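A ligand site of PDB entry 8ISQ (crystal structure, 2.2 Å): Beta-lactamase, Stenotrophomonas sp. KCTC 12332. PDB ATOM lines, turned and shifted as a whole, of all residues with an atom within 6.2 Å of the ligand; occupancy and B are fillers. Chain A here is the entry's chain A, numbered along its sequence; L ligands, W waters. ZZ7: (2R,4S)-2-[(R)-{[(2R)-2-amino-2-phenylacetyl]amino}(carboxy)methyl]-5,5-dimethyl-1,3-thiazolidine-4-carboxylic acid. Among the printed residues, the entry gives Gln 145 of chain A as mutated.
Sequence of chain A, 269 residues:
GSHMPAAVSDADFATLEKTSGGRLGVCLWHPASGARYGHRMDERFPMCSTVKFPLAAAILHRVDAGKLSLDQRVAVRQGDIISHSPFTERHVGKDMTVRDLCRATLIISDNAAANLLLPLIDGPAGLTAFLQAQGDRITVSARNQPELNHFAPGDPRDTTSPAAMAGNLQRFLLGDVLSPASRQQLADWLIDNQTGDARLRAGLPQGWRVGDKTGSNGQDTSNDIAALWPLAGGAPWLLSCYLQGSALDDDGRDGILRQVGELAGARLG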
ATOM      1  N   MET A  47      -4.069  17.560  29.472  1.00  0.00           N
ATOM      2  CA  MET A  47      -2.757  17.369  30.076  1.00  0.00           C
ATOM      3  C   MET A  47      -1.709  16.963  29.050  1.00  0.00           C
ATOM      4  O   MET A  47      -0.570  17.429  29.090  1.00  0.00           O
ATOM      5  CB  MET A  47      -2.826  16.285  31.163  1.00  0.00           C
ATOM      6  CG  MET A  47      -3.433  16.745  32.452  1.00  0.00           C
ATOM      7  SD  MET A  47      -3.242  15.508  33.721  1.00  0.00           S
ATOM      8  CE  MET A  47      -4.605  14.404  33.337  1.00  0.00           C
ATOM      9  N   CYS A  48      -2.081  16.073  28.127  1.00  0.00           N
ATOM     10  CA  CYS A  48      -1.103  15.446  27.226  1.00  0.00           C
ATOM     11  C   CYS A  48      -0.086  14.732  28.124  1.00  0.00           C
ATOM     12  O   CYS A  48      -0.466  14.125  29.133  1.00  0.00           O
ATOM     13  CB  CYS A  48      -0.511  16.461  26.247  1.00  0.00           C
ATOM     14  SG  CYS A  48      -1.656  17.139  24.993  1.00  0.00           S
ATOM     15  N   SER A  49       1.207  14.819  27.791  1.00  0.00           N
ATOM     16  CA  SER A  49       2.226  14.085  28.522  1.00  0.00           C
ATOM     17  C   SER A  49       2.490  14.652  29.911  1.00  0.00           C
ATOM     18  O   SER A  49       3.196  13.997  30.680  1.00  0.00           O
ATOM     19  CB  SER A  49       3.528  14.068  27.716  1.00  0.00           C
ATOM     20  OG  SER A  49       3.429  13.108  26.679  1.00  0.00           O
ATOM     21  N   THR A  50       1.951  15.829  30.251  1.00  0.00           N
ATOM     22  CA  THR A  50       2.180  16.345  31.605  1.00  0.00           C
ATOM     23  C   THR A  50       1.511  15.489  32.662  1.00  0.00           C
ATOM     24  O   THR A  50       1.880  15.585  33.827  1.00  0.00           O
ATOM     25  CB  THR A  50       1.699  17.787  31.714  1.00  0.00           C
ATOM     26  OG1 THR A  50       0.277  17.846  31.542  1.00  0.00           O
ATOM     27  CG2 THR A  50       2.393  18.662  30.668  1.00  0.00           C
ATOM     28  N   LYS A  52       2.250  12.647  33.091  1.00  0.00           N
ATOM     29  CA  LYS A  52       3.329  11.806  33.603  1.00  0.00           C
ATOM     30  C   LYS A  52       3.919  12.330  34.901  1.00  0.00           C
ATOM     31  O   LYS A  52       4.450  11.551  35.692  1.00  0.00           O
ATOM     32  CB  LYS A  52       4.414  11.651  32.542  1.00  0.00           C
ATOM     33  CG  LYS A  52       3.945  10.874  31.328  1.00  0.00           C
ATOM     34  CD  LYS A  52       4.859  11.017  30.122  1.00  0.00           C
ATOM     35  CE  LYS A  52       4.265  10.289  28.915  1.00  0.00           C
ATOM     36  NZ  LYS A  52       5.188  10.301  27.757  1.00  0.00           N
ATOM     37  N   SER A  83       4.250   4.206  20.073  1.00  0.00           N
ATOM     38  CA  SER A  83       5.072   5.245  19.468  1.00  0.00           C
ATOM     39  C   SER A  83       5.783   6.091  20.521  1.00  0.00           C
ATOM     40  O   SER A  83       5.265   6.329  21.615  1.00  0.00           O
ATOM     41  CB  SER A  83       4.211   6.154  18.572  1.00  0.00           C
ATOM     42  OG  SER A  83       3.996   5.544  17.308  1.00  0.00           O
ATOM     43  N   HIS A  84       6.994   6.523  20.189  1.00  0.00           N
ATOM     44  CA  HIS A  84       7.793   7.419  21.029  1.00  0.00           C
ATOM     45  C   HIS A  84       8.061   6.818  22.411  1.00  0.00           C
ATOM     46  O   HIS A  84       7.770   7.411  23.449  1.00  0.00           O
ATOM     47  CB  HIS A  84       7.127   8.787  21.152  1.00  0.00           C
ATOM     48  CG  HIS A  84       8.011   9.807  21.774  1.00  0.00           C
ATOM     49  ND1 HIS A  84       8.255   9.842  23.136  1.00  0.00           N
ATOM     50  CD2 HIS A  84       8.747  10.806  21.237  1.00  0.00           C
ATOM     51  CE1 HIS A  84       9.094  10.827  23.401  1.00  0.00           C
ATOM     52  NE2 HIS A  84       9.403  11.431  22.267  1.00  0.00           N
ATOM     53  N   ILE A 108      12.334  11.961  28.948  1.00  0.00           N
ATOM     54  CA  ILE A 108      12.235  11.892  27.503  1.00  0.00           C
ATOM     55  C   ILE A 108      10.822  11.610  27.027  1.00  0.00           C
ATOM     56  O   ILE A 108      10.579  11.546  25.817  1.00  0.00           O
ATOM     57  CB  ILE A 108      13.232  10.860  26.921  1.00  0.00           C
ATOM     58  CG1 ILE A 108      13.482  11.110  25.417  1.00  0.00           C
ATOM     59  CG2 ILE A 108      12.773   9.427  27.208  1.00  0.00           C
ATOM     60  CD1 ILE A 108      13.927  12.545  25.082  1.00  0.00           C
ATOM     61  N   SER A 109       9.863  11.471  27.949  1.00  0.00           N
ATOM     62  CA  SER A 109       8.464  11.196  27.627  1.00  0.00           C
ATOM     63  C   SER A 109       8.328   9.852  26.898  1.00  0.00           C
ATOM     64  O   SER A 109       7.715   9.756  25.826  1.00  0.00           O
ATOM     65  CB  SER A 109       7.847  12.348  26.827  1.00  0.00           C
ATOM     66  OG  SER A 109       6.550  12.655  27.316  1.00  0.00           O
ATOM     67  N   ASN A 111       6.455   6.824  26.242  1.00  0.00           N
ATOM     68  CA  ASN A 111       5.017   6.616  26.365  1.00  0.00           C
ATOM     69  C   ASN A 111       4.688   5.236  26.916  1.00  0.00           C
ATOM     70  O   ASN A 111       3.785   5.095  27.755  1.00  0.00           O
ATOM     71  CB  ASN A 111       4.332   6.803  25.014  1.00  0.00           C
ATOM     72  CG  ASN A 111       4.092   8.242  24.684  1.00  0.00           C
ATOM     73  OD1 ASN A 111       3.870   9.070  25.581  1.00  0.00           O
ATOM     74  ND2 ASN A 111       4.140   8.581  23.405  1.00  0.00           N
ATOM     75  N   GLN A 145      -1.845   5.817  27.357  1.00  0.00           N
ATOM     76  CA  GLN A 145      -1.330   6.337  26.096  1.00  0.00           C
ATOM     77  C   GLN A 145      -1.683   5.380  24.962  1.00  0.00           C
ATOM     78  O   GLN A 145      -1.685   4.163  25.167  1.00  0.00           O
ATOM     79  CB  GLN A 145       0.195   6.513  26.168  1.00  0.00           C
ATOM     80  CG  GLN A 145       0.644   7.653  27.067  1.00  0.00           C
ATOM     81  CD  GLN A 145       0.549   8.987  26.384  1.00  0.00           C
ATOM     82  OE1 GLN A 145      -0.038   9.113  25.317  1.00  0.00           O
ATOM     83  NE2 GLN A 145       1.158  10.003  26.984  1.00  0.00           N
ATOM     84  N   PRO A 146      -1.982   5.883  23.759  1.00  0.00           N
ATOM     85  CA  PRO A 146      -1.929   7.285  23.339  1.00  0.00           C
ATOM     86  C   PRO A 146      -3.231   8.062  23.534  1.00  0.00           C
ATOM     87  O   PRO A 146      -3.231   9.274  23.287  1.00  0.00           O
ATOM     88  CB  PRO A 146      -1.619   7.188  21.841  1.00  0.00           C
ATOM     89  CG  PRO A 146      -2.396   5.928  21.426  1.00  0.00           C
ATOM     90  CD  PRO A 146      -2.382   4.998  22.632  1.00  0.00           C
ATOM     91  N   LEU A 148      -4.910   9.218  25.938  1.00  0.00           N
ATOM     92  CA  LEU A 148      -5.021  10.335  26.870  1.00  0.00           C
ATOM     93  C   LEU A 148      -4.757  11.680  26.196  1.00  0.00           C
ATOM     94  O   LEU A 148      -5.054  12.720  26.794  1.00  0.00           O
ATOM     95  CB  LEU A 148      -4.084  10.119  28.054  1.00  0.00           C
ATOM     96  CG  LEU A 148      -2.569  10.147  27.882  1.00  0.00           C
ATOM     97  CD1 LEU A 148      -2.033  11.571  27.823  1.00  0.00           C
ATOM     98  CD2 LEU A 148      -1.928   9.384  29.042  1.00  0.00           C
ATOM     99  N   ASN A 149      -4.197  11.685  24.984  1.00  0.00           N
ATOM    100  CA  ASN A 149      -3.942  12.937  24.296  1.00  0.00           C
ATOM    101  C   ASN A 149      -5.155  13.473  23.542  1.00  0.00           C
ATOM    102  O   ASN A 149      -5.099  14.590  23.027  1.00  0.00           O
ATOM    103  CB  ASN A 149      -2.759  12.771  23.339  1.00  0.00           C
ATOM    104  CG  ASN A 149      -1.441  12.906  24.060  1.00  0.00           C
ATOM    105  OD1 ASN A 149      -1.034  14.012  24.405  1.00  0.00           O
ATOM    106  ND2 ASN A 149      -0.775  11.778  24.310  1.00  0.00           N
ATOM    107  N   THR A 195      13.198  17.606  27.047  1.00  0.00           N
ATOM    108  CA  THR A 195      12.252  17.995  26.007  1.00  0.00           C
ATOM    109  C   THR A 195      11.827  19.450  26.072  1.00  0.00           C
ATOM    110  O   THR A 195      10.933  19.855  25.311  1.00  0.00           O
ATOM    111  CB  THR A 195      11.003  17.112  26.074  1.00  0.00           C
ATOM    112  OG1 THR A 195      10.371  17.311  27.339  1.00  0.00           O
ATOM    113  CG2 THR A 195      11.375  15.645  25.914  1.00  0.00           C
ATOM    114  N   ARG A 199      11.416  25.750  25.196  1.00  0.00           N
ATOM    115  CA  ARG A 199      10.114  26.103  25.777  1.00  0.00           C
ATOM    116  C   ARG A 199      10.358  27.065  26.937  1.00  0.00           C
ATOM    117  O   ARG A 199      11.102  28.036  26.749  1.00  0.00           O
ATOM    118  CB  ARG A 199       9.361  24.822  26.092  1.00  0.00           C
ATOM    119  CG  ARG A 199       8.895  24.115  24.833  1.00  0.00           C
ATOM    120  CD  ARG A 199       8.743  22.611  24.992  1.00  0.00           C
ATOM    121  NE  ARG A 199       7.950  22.049  23.896  1.00  0.00           N
ATOM    122  CZ  ARG A 199       7.696  20.762  23.727  1.00  0.00           C
ATOM    123  NH1 ARG A 199       8.180  19.866  24.569  1.00  0.00           N
ATOM    124  NH2 ARG A 199       6.939  20.356  22.716  1.00  0.00           N
ATOM    125  N   LYS A 213       8.299  19.457  32.877  1.00  0.00           N
ATOM    126  CA  LYS A 213       7.728  18.320  32.144  1.00  0.00           C
ATOM    127  C   LYS A 213       6.815  18.881  31.063  1.00  0.00           C
ATOM    128  O   LYS A 213       5.978  19.745  31.342  1.00  0.00           O
ATOM    129  CB  LYS A 213       6.914  17.387  33.051  1.00  0.00           C
ATOM    130  CG  LYS A 213       6.319  16.192  32.289  1.00  0.00           C
ATOM    131  CD  LYS A 213       7.449  15.333  31.744  1.00  0.00           C
ATOM    132  CE  LYS A 213       6.990  14.259  30.766  1.00  0.00           C
ATOM    133  NZ  LYS A 213       6.799  14.809  29.421  1.00  0.00           N
ATOM    134  N   THR A 214       6.964  18.381  29.839  1.00  0.00           N
ATOM    135  CA  THR A 214       6.270  18.908  28.672  1.00  0.00           C
ATOM    136  C   THR A 214       5.225  17.929  28.159  1.00  0.00           C
ATOM    137  O   THR A 214       5.099  16.792  28.621  1.00  0.00           O
ATOM    138  CB  THR A 214       7.265  19.229  27.565  1.00  0.00           C
ATOM    139  OG1 THR A 214       8.023  18.050  27.280  1.00  0.00           O
ATOM    140  CG2 THR A 214       8.224  20.355  27.985  1.00  0.00           C
ATOM    141  N   GLY A 215       4.467  18.409  27.178  1.00  0.00           N
ATOM    142  CA  GLY A 215       3.622  17.554  26.377  1.00  0.00           C
ATOM    143  C   GLY A 215       3.252  18.295  25.117  1.00  0.00           C
ATOM    144  O   GLY A 215       3.330  19.524  25.057  1.00  0.00           O
ATOM    145  N   SER A 216       2.874  17.525  24.086  1.00  0.00           N
ATOM    146  CA  SER A 216       2.440  18.052  22.797  1.00  0.00           C
ATOM    147  C   SER A 216       1.609  16.997  22.092  1.00  0.00           C
ATOM    148  O   SER A 216       1.923  15.808  22.169  1.00  0.00           O
ATOM    149  CB  SER A 216       3.642  18.434  21.915  1.00  0.00           C
ATOM    150  OG  SER A 216       3.206  18.864  20.628  1.00  0.00           O
ATOM    151  N   ASN A 217       0.539  17.423  21.422  1.00  0.00           N
ATOM    152  CA  ASN A 217      -0.210  16.482  20.588  1.00  0.00           C
ATOM    153  C   ASN A 217       0.258  16.480  19.138  1.00  0.00           C
ATOM    154  O   ASN A 217      -0.322  15.770  18.309  1.00  0.00           O
ATOM    155  CB  ASN A 217      -1.729  16.752  20.666  1.00  0.00           C
ATOM    156  CG  ASN A 217      -2.151  18.010  19.930  1.00  0.00           C
ATOM    157  OD1 ASN A 217      -1.321  18.799  19.458  1.00  0.00           O
ATOM    158  ND2 ASN A 217      -3.467  18.221  19.862  1.00  0.00           N
ATOM    159  N   GLY A 218       1.294  17.249  18.820  1.00  0.00           N
ATOM    160  CA  GLY A 218       1.865  17.244  17.495  1.00  0.00           C
ATOM    161  C   GLY A 218       1.114  18.055  16.443  1.00  0.00           C
ATOM    162  O   GLY A 218       1.526  18.036  15.279  1.00  0.00           O
ATOM    163  N   GLN A 219       0.056  18.759  16.809  1.00  0.00           N
ATOM    164  CA  GLN A 219      -0.725  19.505  15.827  1.00  0.00           C
ATOM    165  C   GLN A 219      -1.128  20.884  16.336  1.00  0.00           C
ATOM    166  O   GLN A 219      -0.962  21.879  15.629  1.00  0.00           O
ATOM    167  CB  GLN A 219      -1.986  18.730  15.419  1.00  0.00           C
ATOM    168  CG  GLN A 219      -1.735  17.353  14.828  1.00  0.00           C
ATOM    169  CD  GLN A 219      -0.995  17.391  13.497  1.00  0.00           C
ATOM    170  OE1 GLN A 219      -0.981  18.411  12.798  1.00  0.00           O
ATOM    171  NE2 GLN A 219      -0.401  16.276  13.127  1.00  0.00           N
ATOM    172  N   SER A 222       0.623  22.400  23.093  1.00  0.00           N
ATOM    173  CA  SER A 222       1.899  22.222  23.770  1.00  0.00           C
ATOM    174  C   SER A 222       1.784  22.747  25.190  1.00  0.00           C
ATOM    175  O   SER A 222       1.290  23.854  25.413  1.00  0.00           O
ATOM    176  CB  SER A 222       3.032  22.936  23.017  1.00  0.00           C
ATOM    177  OG  SER A 222       3.304  22.298  21.784  1.00  0.00           O
ATOM    178  N   ASN A 223       2.253  21.935  26.140  1.00  0.00           N
ATOM    179  CA  ASN A 223       2.187  22.212  27.571  1.00  0.00           C
ATOM    180  C   ASN A 223       3.587  22.106  28.167  1.00  0.00           C
ATOM    181  O   ASN A 223       4.418  21.330  27.694  1.00  0.00           O
ATOM    182  CB  ASN A 223       1.289  21.225  28.313  1.00  0.00           C
ATOM    183  CG  ASN A 223      -0.044  21.057  27.655  1.00  0.00           C
ATOM    184  OD1 ASN A 223      -0.615  22.008  27.131  1.00  0.00           O
ATOM    185  ND2 ASN A 223      -0.563  19.839  27.679  1.00  0.00           N
ATOM    186  N   ASP A 250       4.369  23.157  16.456  1.00  0.00           N
ATOM    187  CA  ASP A 250       5.165  22.907  17.660  1.00  0.00           C
ATOM    188  C   ASP A 250       6.252  23.960  17.842  1.00  0.00           C
ATOM    189  O   ASP A 250       6.443  24.464  18.953  1.00  0.00           O
ATOM    190  CB  ASP A 250       5.761  21.507  17.618  1.00  0.00           C
ATOM    191  CG  ASP A 250       4.792  20.468  18.166  1.00  0.00           C
ATOM    192  OD1 ASP A 250       3.847  20.090  17.436  1.00  0.00           O
ATOM    193  OD2 ASP A 250       4.943  20.054  19.346  1.00  0.00           O
HETATM  194  O1  ZZ7 L   1       6.858  16.987  25.344  1.00  0.00           O
HETATM  195  C2  ZZ7 L   1       6.552  16.765  24.140  1.00  0.00           C
HETATM  196  O2  ZZ7 L   1       6.837  17.618  23.273  1.00  0.00           O
HETATM  197  C12 ZZ7 L   1       5.900  15.504  23.789  1.00  0.00           C
HETATM  198  C6  ZZ7 L   1       6.989  14.493  23.004  1.00  0.00           C
HETATM  199  C1  ZZ7 L   1       8.364  14.550  23.668  1.00  0.00           C
HETATM  200  C16 ZZ7 L   1       7.126  14.897  21.550  1.00  0.00           C
HETATM  201  S1  ZZ7 L   1       6.229  12.969  23.163  1.00  0.00           S
HETATM  202  N3  ZZ7 L   1       5.658  14.777  24.916  1.00  0.00           N
HETATM  203  C13 ZZ7 L   1       5.487  13.105  24.358  1.00  0.00           C
HETATM  204  C14 ZZ7 L   1       3.925  12.836  24.254  1.00  0.00           C
HETATM  205  C15 ZZ7 L   1       3.193  13.523  25.391  1.00  0.00           C
HETATM  206  O4  ZZ7 L   1       2.607  14.636  25.241  1.00  0.00           O
HETATM  207  N1  ZZ7 L   1       3.387  13.322  23.009  1.00  0.00           N
HETATM  208  C3  ZZ7 L   1       3.113  12.380  21.943  1.00  0.00           C
HETATM  209  O3  ZZ7 L   1       3.351  11.229  22.119  1.00  0.00           O
HETATM  210  C4  ZZ7 L   1       2.532  12.887  20.626  1.00  0.00           C
HETATM  211  N2  ZZ7 L   1       1.800  11.849  19.928  1.00  0.00           N
HETATM  212  C5  ZZ7 L   1       3.703  13.412  19.818  1.00  0.00           C
HETATM  213  C7  ZZ7 L   1       4.745  12.570  19.463  1.00  0.00           C
HETATM  214  C8  ZZ7 L   1       5.813  13.062  18.749  1.00  0.00           C
HETATM  215  C9  ZZ7 L   1       5.861  14.403  18.371  1.00  0.00           C
HETATM  216  C10 ZZ7 L   1       4.826  15.251  18.736  1.00  0.00           C
HETATM  217  C11 ZZ7 L   1       3.750  14.747  19.452  1.00  0.00           C
HETATM  218  O   HOH W   1      -0.805  13.280  19.457  1.00  0.00           O
HETATM  219  O   HOH W   2       1.373  10.596  17.423  1.00  0.00           O
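The backbone NH of Gly 215 is in hydrogen-bond range of an oxygen (O1) of the ligand (3.3 Å).
The backbone NH (N) of Ser 49 lies close to an oxygen (O4) of the ligand (2.9 Å).
OG1 of Thr 214 sits at hydrogen-bond distance from O1 of the ligand (2.5 Å).
O3 of the ligand is in hydrogen-bond range of ND2 of Asn 111 (3.0 Å).
The backbone NH (N) of Ser 216 is in hydrogen-bond range of an oxygen (O4) of the ligand, at 3.1 Å.
O of Ser 216 is in hydrogen-bond range of N1 of the ligand (3.0 Å).
S1 of the ligand lies close to NE2 of His 84.
The side-chain hydroxyl (OG) of Ser 49 is bonded to a carbon (C15) of the ligand (1.4 Å).
O2 of the ligand lies within salt-bridge range of NH2 of Arg 199, at 2.8 Å.
A nitrogen (N3) of the ligand sits close to the side-chain hydroxyl of Ser 109, 3.3 Å away.
OG of Ser 109 lies within hydrogen-bond range of NZ of Lys 213.
The backbone carbonyl oxygen (O) of Ser 83 lies within hydrogen-bond range of the side-chain amide nitrogen (ND2) of Asn 111, 3.1 Å away.
OD2 of Asp 250 is in salt-bridge range of NH2 of Arg 199 (3.9 Å).
O of Ser 109 is in hydrogen-bond range of ND1 of His 84, at 2.7 Å.
The side-chain carboxylate (OD2) of Asp 250 sits at hydrogen-bond distance from the side-chain hydroxyl (OG) of Ser 216.
The side-chain amide oxygen (OD1) of Asn 111 sits at hydrogen-bond distance from the side-chain amide nitrogen (NE2) of Gln 145 (3.2 Å).
NH1 of Arg 199 lies within hydrogen-bond range of O of Thr 195.
The side-chain hydroxyl of Ser 49 is in hydrogen-bond range of the side-chain hydroxyl of Ser 109, 3.2 Å away.
Residues that only touch the ligand: Gly 218, Cys 48, Asn 149, Asn 217 and Thr 195.
Hydrophobic or aromatic side chains that line the ligand: His 84.
Within 4 Å of the ligand: Cys 48, Ser 49, His 84, Ser 109, Asn 111, Asn 149, Thr 195, Arg 199, Thr 214, Gly 215, Ser 216, Asn 217 and Gly 218.
The nearest printed residue that does not touch the ligand is Ile 108 (4.3 Å).
Water W1 bridges O of Asn 217 (2.8 Å) and N2 of the ligand (3.0 Å).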
